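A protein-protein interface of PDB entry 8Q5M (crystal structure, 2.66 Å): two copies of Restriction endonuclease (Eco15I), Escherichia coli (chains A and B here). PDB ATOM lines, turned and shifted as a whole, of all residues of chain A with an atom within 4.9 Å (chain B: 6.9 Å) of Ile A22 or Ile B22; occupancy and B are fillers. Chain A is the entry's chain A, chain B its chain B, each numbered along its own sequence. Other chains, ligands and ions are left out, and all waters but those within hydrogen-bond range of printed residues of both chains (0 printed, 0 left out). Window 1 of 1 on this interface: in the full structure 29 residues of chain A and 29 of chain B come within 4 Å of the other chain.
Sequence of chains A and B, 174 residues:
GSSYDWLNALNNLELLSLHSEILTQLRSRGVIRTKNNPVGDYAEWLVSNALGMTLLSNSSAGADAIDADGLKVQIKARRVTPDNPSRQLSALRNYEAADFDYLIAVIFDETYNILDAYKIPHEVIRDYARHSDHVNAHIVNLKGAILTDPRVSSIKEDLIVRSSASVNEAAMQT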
ATOM      1  N   LEU A   7     -26.494   3.372  29.572  1.00  0.00           N
ATOM      2  CA  LEU A   7     -27.522   4.383  29.340  1.00  0.00           C
ATOM      3  C   LEU A   7     -28.473   4.498  30.520  1.00  0.00           C
ATOM      4  O   LEU A   7     -29.109   5.543  30.697  1.00  0.00           O
ATOM      5  CB  LEU A   7     -28.316   4.066  28.076  1.00  0.00           C
ATOM      6  CG  LEU A   7     -27.620   4.216  26.734  1.00  0.00           C
ATOM      7  CD1 LEU A   7     -28.531   3.700  25.651  1.00  0.00           C
ATOM      8  CD2 LEU A   7     -27.258   5.667  26.493  1.00  0.00           C
ATOM      9  N   LEU A  15     -29.859  11.789  27.924  1.00  0.00           N
ATOM     10  CA  LEU A  15     -30.278  10.903  26.837  1.00  0.00           C
ATOM     11  C   LEU A  15     -30.657  11.687  25.586  1.00  0.00           C
ATOM     12  O   LEU A  15     -30.209  11.371  24.477  1.00  0.00           O
ATOM     13  CB  LEU A  15     -31.449  10.042  27.304  1.00  0.00           C
ATOM     14  CG  LEU A  15     -31.071   8.942  28.292  1.00  0.00           C
ATOM     15  CD1 LEU A  15     -32.304   8.262  28.825  1.00  0.00           C
ATOM     16  CD2 LEU A  15     -30.180   7.915  27.595  1.00  0.00           C
ATOM     17  N   LEU A  18     -27.584  13.464  23.980  1.00  0.00           N
ATOM     18  CA  LEU A  18     -26.779  12.491  23.252  1.00  0.00           C
ATOM     19  C   LEU A  18     -27.469  12.065  21.963  1.00  0.00           C
ATOM     20  O   LEU A  18     -26.830  11.944  20.915  1.00  0.00           O
ATOM     21  CB  LEU A  18     -26.488  11.297  24.159  1.00  0.00           C
ATOM     22  CG  LEU A  18     -25.651  10.161  23.583  1.00  0.00           C
ATOM     23  CD1 LEU A  18     -24.304  10.640  23.013  1.00  0.00           C
ATOM     24  CD2 LEU A  18     -25.464   9.118  24.673  1.00  0.00           C
ATOM     25  N   HIS A  19     -28.779  11.825  22.027  1.00  0.00           N
ATOM     26  CA  HIS A  19     -29.541  11.488  20.829  1.00  0.00           C
ATOM     27  C   HIS A  19     -29.332  12.512  19.721  1.00  0.00           C
ATOM     28  O   HIS A  19     -29.180  12.158  18.548  1.00  0.00           O
ATOM     29  CB  HIS A  19     -31.027  11.389  21.170  1.00  0.00           C
ATOM     30  CG  HIS A  19     -31.925  11.687  20.010  1.00  0.00           C
ATOM     31  ND1 HIS A  19     -32.514  12.924  19.844  1.00  0.00           N
ATOM     32  CD2 HIS A  19     -32.326  10.933  18.957  1.00  0.00           C
ATOM     33  CE1 HIS A  19     -33.246  12.918  18.745  1.00  0.00           C
ATOM     34  NE2 HIS A  19     -33.150  11.723  18.188  1.00  0.00           N
ATOM     35  N   SER A  20     -29.357  13.796  20.069  1.00  0.00           N
ATOM     36  CA  SER A  20     -29.268  14.825  19.040  1.00  0.00           C
ATOM     37  C   SER A  20     -27.845  14.963  18.516  1.00  0.00           C
ATOM     38  O   SER A  20     -27.639  15.302  17.346  1.00  0.00           O
ATOM     39  CB  SER A  20     -29.795  16.153  19.584  1.00  0.00           C
ATOM     40  OG  SER A  20     -31.187  16.051  19.831  1.00  0.00           O
ATOM     41  N   GLU A  21     -26.857  14.731  19.380  1.00  0.00           N
ATOM     42  CA  GLU A  21     -25.443  14.807  19.008  1.00  0.00           C
ATOM     43  C   GLU A  21     -25.032  13.647  18.112  1.00  0.00           C
ATOM     44  O   GLU A  21     -24.148  13.787  17.259  1.00  0.00           O
ATOM     45  CB  GLU A  21     -24.601  14.862  20.277  1.00  0.00           C
ATOM     46  CG  GLU A  21     -24.941  16.114  21.070  1.00  0.00           C
ATOM     47  CD  GLU A  21     -24.011  17.262  20.813  1.00  0.00           C
ATOM     48  OE1 GLU A  21     -23.228  17.198  19.844  1.00  0.00           O
ATOM     49  OE2 GLU A  21     -24.149  18.282  21.507  1.00  0.00           O
ATOM     50  N   ILE A  22     -25.571  12.465  18.379  1.00  0.00           N
ATOM     51  CA  ILE A  22     -25.437  11.314  17.496  1.00  0.00           C
ATOM     52  C   ILE A  22     -25.936  11.662  16.097  1.00  0.00           C
ATOM     53  O   ILE A  22     -25.252  11.403  15.102  1.00  0.00           O
ATOM     54  CB  ILE A  22     -26.176  10.103  18.086  1.00  0.00           C
ATOM     55  CG1 ILE A  22     -25.428   9.634  19.338  1.00  0.00           C
ATOM     56  CG2 ILE A  22     -26.280   8.995  17.063  1.00  0.00           C
ATOM     57  CD1 ILE A  22     -26.169   8.620  20.170  1.00  0.00           C
ATOM     58  N   LEU A  23     -27.135  12.245  16.008  1.00  0.00           N
ATOM     59  CA  LEU A  23     -27.691  12.581  14.701  1.00  0.00           C
ATOM     60  C   LEU A  23     -26.891  13.680  14.020  1.00  0.00           C
ATOM     61  O   LEU A  23     -26.745  13.668  12.793  1.00  0.00           O
ATOM     62  CB  LEU A  23     -29.153  13.007  14.829  1.00  0.00           C
ATOM     63  CG  LEU A  23     -30.076  11.890  15.301  1.00  0.00           C
ATOM     64  CD1 LEU A  23     -31.512  12.360  15.403  1.00  0.00           C
ATOM     65  CD2 LEU A  23     -29.950  10.687  14.379  1.00  0.00           C
ATOM     66  N   THR A  24     -26.372  14.635  14.788  1.00  0.00           N
ATOM     67  CA  THR A  24     -25.498  15.640  14.202  1.00  0.00           C
ATOM     68  C   THR A  24     -24.228  14.999  13.664  1.00  0.00           C
ATOM     69  O   THR A  24     -23.759  15.356  12.579  1.00  0.00           O
ATOM     70  CB  THR A  24     -25.183  16.724  15.228  1.00  0.00           C
ATOM     71  OG1 THR A  24     -26.381  17.453  15.522  1.00  0.00           O
ATOM     72  CG2 THR A  24     -24.111  17.668  14.705  1.00  0.00           C
ATOM     73  N   GLN A  25     -23.663  14.046  14.407  1.00  0.00           N
ATOM     74  CA  GLN A  25     -22.467  13.346  13.951  1.00  0.00           C
ATOM     75  C   GLN A  25     -22.723  12.609  12.643  1.00  0.00           C
ATOM     76  O   GLN A  25     -21.876  12.605  11.739  1.00  0.00           O
ATOM     77  CB  GLN A  25     -21.987  12.391  15.042  1.00  0.00           C
ATOM     78  CG  GLN A  25     -20.712  11.628  14.725  1.00  0.00           C
ATOM     79  CD  GLN A  25     -19.491  12.521  14.667  1.00  0.00           C
ATOM     80  OE1 GLN A  25     -18.697  12.436  13.728  1.00  0.00           O
ATOM     81  NE2 GLN A  25     -19.356  13.414  15.637  1.00  0.00           N
ATOM     82  N   LEU A  26     -23.875  11.948  12.538  1.00  0.00           N
ATOM     83  CA  LEU A  26     -24.202  11.232  11.315  1.00  0.00           C
ATOM     84  C   LEU A  26     -24.430  12.202  10.158  1.00  0.00           C
ATOM     85  O   LEU A  26     -24.009  11.930   9.028  1.00  0.00           O
ATOM     86  CB  LEU A  26     -25.423  10.350  11.551  1.00  0.00           C
ATOM     87  CG  LEU A  26     -25.238   9.152  12.478  1.00  0.00           C
ATOM     88  CD1 LEU A  26     -26.591   8.567  12.810  1.00  0.00           C
ATOM     89  CD2 LEU A  26     -24.345   8.105  11.851  1.00  0.00           C
ATOM     90  N   TYR B   4     -19.120  15.786  23.532  1.00  0.00           N
ATOM     91  CA  TYR B   4     -19.565  14.776  22.582  1.00  0.00           C
ATOM     92  C   TYR B   4     -18.587  14.591  21.426  1.00  0.00           C
ATOM     93  O   TYR B   4     -18.980  14.079  20.373  1.00  0.00           O
ATOM     94  CB  TYR B   4     -20.960  15.150  22.056  1.00  0.00           C
ATOM     95  CG  TYR B   4     -21.996  15.244  23.150  1.00  0.00           C
ATOM     96  CD1 TYR B   4     -22.657  14.113  23.601  1.00  0.00           C
ATOM     97  CD2 TYR B   4     -22.301  16.463  23.745  1.00  0.00           C
ATOM     98  CE1 TYR B   4     -23.599  14.189  24.607  1.00  0.00           C
ATOM     99  CE2 TYR B   4     -23.240  16.551  24.760  1.00  0.00           C
ATOM    100  CZ  TYR B   4     -23.885  15.411  25.186  1.00  0.00           C
ATOM    101  OH  TYR B   4     -24.820  15.483  26.186  1.00  0.00           O
ATOM    102  N   TRP B   6     -16.210  12.476  21.514  1.00  0.00           N
ATOM    103  CA  TRP B   6     -15.922  11.052  21.465  1.00  0.00           C
ATOM    104  C   TRP B   6     -16.802  10.342  20.450  1.00  0.00           C
ATOM    105  O   TRP B   6     -16.490   9.214  20.055  1.00  0.00           O
ATOM    106  CB  TRP B   6     -16.103  10.440  22.850  1.00  0.00           C
ATOM    107  CG  TRP B   6     -17.460  10.642  23.422  1.00  0.00           C
ATOM    108  CD1 TRP B   6     -17.920  11.751  24.071  1.00  0.00           C
ATOM    109  CD2 TRP B   6     -18.524   9.685  23.461  1.00  0.00           C
ATOM    110  NE1 TRP B   6     -19.218  11.557  24.476  1.00  0.00           N
ATOM    111  CE2 TRP B   6     -19.610  10.294  24.119  1.00  0.00           C
ATOM    112  CE3 TRP B   6     -18.665   8.375  22.996  1.00  0.00           C
ATOM    113  CZ2 TRP B   6     -20.816   9.642  24.322  1.00  0.00           C
ATOM    114  CZ3 TRP B   6     -19.863   7.728  23.198  1.00  0.00           C
ATOM    115  CH2 TRP B   6     -20.925   8.361  23.855  1.00  0.00           C
ATOM    116  N   LEU B   7     -17.900  10.977  20.037  1.00  0.00           N
ATOM    117  CA  LEU B   7     -18.748  10.415  18.995  1.00  0.00           C
ATOM    118  C   LEU B   7     -17.989  10.267  17.683  1.00  0.00           C
ATOM    119  O   LEU B   7     -18.325   9.404  16.865  1.00  0.00           O
ATOM    120  CB  LEU B   7     -19.988  11.291  18.804  1.00  0.00           C
ATOM    121  CG  LEU B   7     -20.989  11.317  19.967  1.00  0.00           C
ATOM    122  CD1 LEU B   7     -22.097  12.328  19.711  1.00  0.00           C
ATOM    123  CD2 LEU B   7     -21.567   9.941  20.279  1.00  0.00           C
ATOM    124  N   LEU B  10     -16.741   6.640  16.934  1.00  0.00           N
ATOM    125  CA  LEU B  10     -17.628   5.512  16.700  1.00  0.00           C
ATOM    126  C   LEU B  10     -17.889   5.352  15.211  1.00  0.00           C
ATOM    127  O   LEU B  10     -17.848   6.319  14.445  1.00  0.00           O
ATOM    128  CB  LEU B  10     -18.948   5.675  17.457  1.00  0.00           C
ATOM    129  CG  LEU B  10     -18.980   5.291  18.938  1.00  0.00           C
ATOM    130  CD1 LEU B  10     -18.024   6.133  19.752  1.00  0.00           C
ATOM    131  CD2 LEU B  10     -20.394   5.448  19.477  1.00  0.00           C
ATOM    132  N   GLU B  14     -22.396   1.707  15.101  1.00  0.00           N
ATOM    133  CA  GLU B  14     -22.445   1.899  16.552  1.00  0.00           C
ATOM    134  C   GLU B  14     -23.287   3.113  16.919  1.00  0.00           C
ATOM    135  O   GLU B  14     -24.041   3.080  17.896  1.00  0.00           O
ATOM    136  CB  GLU B  14     -21.040   2.066  17.129  1.00  0.00           C
ATOM    137  CG  GLU B  14     -20.176   0.828  17.115  1.00  0.00           C
ATOM    138  CD  GLU B  14     -18.718   1.147  17.395  1.00  0.00           C
ATOM    139  OE1 GLU B  14     -18.209   2.132  16.816  1.00  0.00           O
ATOM    140  OE2 GLU B  14     -18.087   0.427  18.198  1.00  0.00           O
ATOM    141  N   LEU B  15     -23.122   4.208  16.176  1.00  0.00           N
ATOM    142  CA  LEU B  15     -23.963   5.384  16.360  1.00  0.00           C
ATOM    143  C   LEU B  15     -25.435   5.033  16.200  1.00  0.00           C
ATOM    144  O   LEU B  15     -26.281   5.482  16.983  1.00  0.00           O
ATOM    145  CB  LEU B  15     -23.554   6.471  15.365  1.00  0.00           C
ATOM    146  CG  LEU B  15     -22.220   7.172  15.630  1.00  0.00           C
ATOM    147  CD1 LEU B  15     -21.886   8.141  14.511  1.00  0.00           C
ATOM    148  CD2 LEU B  15     -22.252   7.900  16.978  1.00  0.00           C
ATOM    149  N   LEU B  16     -25.759   4.239  15.182  1.00  0.00           N
ATOM    150  CA  LEU B  16     -27.150   3.903  14.915  1.00  0.00           C
ATOM    151  C   LEU B  16     -27.708   2.964  15.975  1.00  0.00           C
ATOM    152  O   LEU B  16     -28.856   3.121  16.409  1.00  0.00           O
ATOM    153  CB  LEU B  16     -27.257   3.284  13.532  1.00  0.00           C
ATOM    154  CG  LEU B  16     -27.331   4.323  12.421  1.00  0.00           C
ATOM    155  CD1 LEU B  16     -26.897   3.652  11.130  1.00  0.00           C
ATOM    156  CD2 LEU B  16     -28.721   4.895  12.308  1.00  0.00           C
ATOM    157  N   SER B  17     -26.916   1.978  16.402  1.00  0.00           N
ATOM    158  CA  SER B  17     -27.356   1.101  17.483  1.00  0.00           C
ATOM    159  C   SER B  17     -27.500   1.873  18.787  1.00  0.00           C
ATOM    160  O   SER B  17     -28.451   1.650  19.543  1.00  0.00           O
ATOM    161  CB  SER B  17     -26.391  -0.068  17.642  1.00  0.00           C
ATOM    162  OG  SER B  17     -26.296  -0.804  16.433  1.00  0.00           O
ATOM    163  N   LEU B  18     -26.562   2.776  19.074  1.00  0.00           N
ATOM    164  CA  LEU B  18     -26.671   3.588  20.281  1.00  0.00           C
ATOM    165  C   LEU B  18     -27.908   4.472  20.221  1.00  0.00           C
ATOM    166  O   LEU B  18     -28.618   4.631  21.217  1.00  0.00           O
ATOM    167  CB  LEU B  18     -25.410   4.434  20.459  1.00  0.00           C
ATOM    168  CG  LEU B  18     -25.314   5.326  21.692  1.00  0.00           C
ATOM    169  CD1 LEU B  18     -25.511   4.503  22.961  1.00  0.00           C
ATOM    170  CD2 LEU B  18     -23.958   6.040  21.715  1.00  0.00           C
ATOM    171  N   HIS B  19     -28.165   5.062  19.056  1.00  0.00           N
ATOM    172  CA  HIS B  19     -29.341   5.899  18.866  1.00  0.00           C
ATOM    173  C   HIS B  19     -30.629   5.177  19.236  1.00  0.00           C
ATOM    174  O   HIS B  19     -31.528   5.771  19.837  1.00  0.00           O
ATOM    175  CB  HIS B  19     -29.371   6.373  17.417  1.00  0.00           C
ATOM    176  CG  HIS B  19     -30.711   6.837  16.958  1.00  0.00           C
ATOM    177  ND1 HIS B  19     -31.231   8.061  17.315  1.00  0.00           N
ATOM    178  CD2 HIS B  19     -31.606   6.271  16.112  1.00  0.00           C
ATOM    179  CE1 HIS B  19     -32.410   8.215  16.737  1.00  0.00           C
ATOM    180  NE2 HIS B  19     -32.659   7.145  16.000  1.00  0.00           N
ATOM    181  N   SER B  20     -30.767   3.919  18.829  1.00  0.00           N
ATOM    182  CA  SER B  20     -32.009   3.202  19.091  1.00  0.00           C
ATOM    183  C   SER B  20     -32.107   2.765  20.545  1.00  0.00           C
ATOM    184  O   SER B  20     -33.207   2.733  21.110  1.00  0.00           O
ATOM    185  CB  SER B  20     -32.118   2.027  18.135  1.00  0.00           C
ATOM    186  OG  SER B  20     -32.249   2.540  16.817  1.00  0.00           O
ATOM    187  N   GLU B  21     -30.968   2.465  21.175  1.00  0.00           N
ATOM    188  CA  GLU B  21     -30.979   2.104  22.583  1.00  0.00           C
ATOM    189  C   GLU B  21     -31.432   3.286  23.423  1.00  0.00           C
ATOM    190  O   GLU B  21     -32.173   3.119  24.397  1.00  0.00           O
ATOM    191  CB  GLU B  21     -29.581   1.672  23.022  1.00  0.00           C
ATOM    192  CG  GLU B  21     -29.001   0.421  22.391  1.00  0.00           C
ATOM    193  CD  GLU B  21     -29.262  -0.813  23.231  1.00  0.00           C
ATOM    194  OE1 GLU B  21     -30.421  -1.006  23.662  1.00  0.00           O
ATOM    195  OE2 GLU B  21     -28.290  -1.557  23.509  1.00  0.00           O
ATOM    196  N   ILE B  22     -30.960   4.484  23.078  1.00  0.00           N
ATOM    197  CA  ILE B  22     -31.445   5.698  23.723  1.00  0.00           C
ATOM    198  C   ILE B  22     -32.960   5.793  23.615  1.00  0.00           C
ATOM    199  O   ILE B  22     -33.659   5.976  24.615  1.00  0.00           O
ATOM    200  CB  ILE B  22     -30.755   6.933  23.122  1.00  0.00           C
ATOM    201  CG1 ILE B  22     -29.277   6.933  23.507  1.00  0.00           C
ATOM    202  CG2 ILE B  22     -31.426   8.192  23.619  1.00  0.00           C
ATOM    203  CD1 ILE B  22     -28.458   7.961  22.781  1.00  0.00           C
ATOM    204  N   LEU B  23     -33.495   5.651  22.406  1.00  0.00           N
ATOM    205  CA  LEU B  23     -34.937   5.785  22.236  1.00  0.00           C
ATOM    206  C   LEU B  23     -35.687   4.658  22.934  1.00  0.00           C
ATOM    207  O   LEU B  23     -36.802   4.866  23.425  1.00  0.00           O
ATOM    208  CB  LEU B  23     -35.268   5.878  20.749  1.00  0.00           C
ATOM    209  CG  LEU B  23     -34.670   7.182  20.211  1.00  0.00           C
ATOM    210  CD1 LEU B  23     -34.959   7.336  18.726  1.00  0.00           C
ATOM    211  CD2 LEU B  23     -35.211   8.357  21.015  1.00  0.00           C
ATOM    212  N   THR B  24     -35.099   3.462  22.987  1.00  0.00           N
ATOM    213  CA  THR B  24     -35.687   2.390  23.782  1.00  0.00           C
ATOM    214  C   THR B  24     -35.686   2.755  25.260  1.00  0.00           C
ATOM    215  O   THR B  24     -36.675   2.527  25.966  1.00  0.00           O
ATOM    216  CB  THR B  24     -34.929   1.081  23.540  1.00  0.00           C
ATOM    217  OG1 THR B  24     -35.146   0.654  22.193  1.00  0.00           O
ATOM    218  CG2 THR B  24     -35.391  -0.009  24.483  1.00  0.00           C
ATOM    219  N   GLN B  25     -34.579   3.332  25.742  1.00  0.00           N
ATOM    220  CA  GLN B  25     -34.477   3.740  27.140  1.00  0.00           C
ATOM    221  C   GLN B  25     -35.520   4.793  27.494  1.00  0.00           C
ATOM    222  O   GLN B  25     -36.177   4.702  28.539  1.00  0.00           O
ATOM    223  CB  GLN B  25     -33.068   4.265  27.414  1.00  0.00           C
ATOM    224  CG  GLN B  25     -32.791   4.628  28.863  1.00  0.00           C
ATOM    225  CD  GLN B  25     -32.684   3.417  29.769  1.00  0.00           C
ATOM    226  OE1 GLN B  25     -33.316   3.358  30.823  1.00  0.00           O
ATOM    227  NE2 GLN B  25     -31.881   2.446  29.361  1.00  0.00           N
ATOM    228  N   LEU B  26     -35.689   5.799  26.630  1.00  0.00           N
ATOM    229  CA  LEU B  26     -36.642   6.873  26.896  1.00  0.00           C
ATOM    230  C   LEU B  26     -38.071   6.361  26.878  1.00  0.00           C
ATOM    231  O   LEU B  26     -38.891   6.749  27.718  1.00  0.00           O
ATOM    232  CB  LEU B  26     -36.478   7.966  25.848  1.00  0.00           C
ATOM    233  CG  LEU B  26     -35.193   8.752  25.977  1.00  0.00           C
ATOM    234  CD1 LEU B  26     -34.963   9.617  24.757  1.00  0.00           C
ATOM    235  CD2 LEU B  26     -35.324   9.585  27.219  1.00  0.00           C
ATOM    236  N   ARG B  27     -38.381   5.500  25.910  1.00  0.00           N
ATOM    237  CA  ARG B  27     -39.705   4.897  25.819  1.00  0.00           C
ATOM    238  C   ARG B  27     -39.996   4.030  27.037  1.00  0.00           C
ATOM    239  O   ARG B  27     -41.144   3.951  27.490  1.00  0.00           O
ATOM    240  CB  ARG B  27     -39.805   4.125  24.509  1.00  0.00           C
ATOM    241  CG  ARG B  27     -41.167   4.123  23.816  1.00  0.00           C
ATOM    242  CD  ARG B  27     -40.874   3.822  22.361  1.00  0.00           C
ATOM    243  NE  ARG B  27     -40.140   2.571  22.214  1.00  0.00           N
ATOM    244  CZ  ARG B  27     -39.269   2.333  21.242  1.00  0.00           C
ATOM    245  NH1 ARG B  27     -38.999   3.247  20.320  1.00  0.00           N
ATOM    246  NH2 ARG B  27     -38.655   1.153  21.194  1.00  0.00           N
ATOM    247  N   SER B  28     -38.974   3.338  27.552  1.00  0.00           N
ATOM    248  CA  SER B  28     -39.149   2.500  28.735  1.00  0.00           C
ATOM    249  C   SER B  28     -39.361   3.338  29.990  1.00  0.00           C
ATOM    250  O   SER B  28     -39.970   2.864  30.955  1.00  0.00           O
ATOM    251  CB  SER B  28     -37.938   1.590  28.920  1.00  0.00           C
ATOM    252  OG  SER B  28     -36.963   2.221  29.739  1.00  0.00           O
ATOM    253  N   ILE B  32     -40.793   9.470  26.192  1.00  0.00           N
ATOM    254  CA  ILE B  32     -41.310   9.536  24.836  1.00  0.00           C
ATOM    255  C   ILE B  32     -42.269   8.369  24.655  1.00  0.00           C
ATOM    256  O   ILE B  32     -42.010   7.257  25.131  1.00  0.00           O
ATOM    257  CB  ILE B  32     -40.200   9.531  23.762  1.00  0.00           C
ATOM    258  CG1 ILE B  32     -39.441   8.209  23.728  1.00  0.00           C
ATOM    259  CG2 ILE B  32     -39.225  10.679  23.983  1.00  0.00           C
ATOM    260  CD1 ILE B  32     -38.377   8.176  22.665  1.00  0.00           C
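The backbone carbonyl oxygen (O) of Gln B25 is in hydrogen-bond range of the side-chain hydroxyl (OG) of Ser B28. A ring nitrogen (ND1) of His A19 is in hydrogen-bond range of the side-chain hydroxyl of Ser A20.
CB of Glu B21 touches CD1 of Leu A7 (3.5 Å). Leu A15 touches Gln B25. Leu A18 touches Leu B7 (CD1 to CD2, 3.9 Å). CD1 of Ile B22 touches CG of Leu A18 (3.7 Å). Glu A21 touches Tyr B4 (OE2 to CD2, 3.4 Å). Ile A22 touches Leu B15. Ile A22 touches Leu B18 (CD1 to CG, 3.7 Å). NE2 of Gln A25 touches CB of Leu B7, 3.9 Å away. Gln A25 touches Leu B15. CD1 of Leu B15 touches CD2 of Leu A26, at 3.6 Å.
Of the printed residues of chain B, Glu A21 touches Tyr B4 (3.4 Å) and Leu B7 (3.5 Å). Ile A22 touches four residues of chain B. Printed residues of chain B within 4 Å of Gln A25: Leu B7 and Leu B15. Ile B22 touches five residues of chain A. The nearest residue of chain B that does not touch Ile A22 is His B19 (4.1 Å). The nearest printed residue of chain A that does not touch Ile B22 is Ser A20 (6.5 Å). The nearest printed residue of chain A that does not touch Leu B18 is Leu A7 (4.1 Å).
Hydrophobic or aromatic side chains of chain A that line the printed part of chain B: Leu A7, Leu A15, Leu A18, His A19, Ile A22 and Leu A26. Along chain A the printed residues that touch a printed residue of chain B span positions 7 to 26. Of the 20 printed residues of chain B, 10 touch a printed residue of chain A. Along chain B the printed residues that touch a printed residue of chain A span positions 4 to 26. Among the printed residues, 20 pairs touch across the chains. Among the printed residues, no Asp or Glu carboxylate lies within 4 Å of a Lys or Arg side-chain nitrogen of the other chain.
Leu A7 touches Glu B21, and with the chains exchanged Glu A21 touches Leu B7. Leu A18 touches Ile B22, and with the chains exchanged Ile A22 touches Leu B18. His A19 touches Ile B22, but with the chains exchanged Ile A22 does not touch His B19 (4.1 Å). Gln A25 touches Leu B7, but with the chains exchanged Leu A7 does not touch Gln B25 (4.1 Å). 11 positions are printed for both chains. Of the 20 pairs that touch across the chains among the printed residues, 14 have their exchanged pair printed and touching as well.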
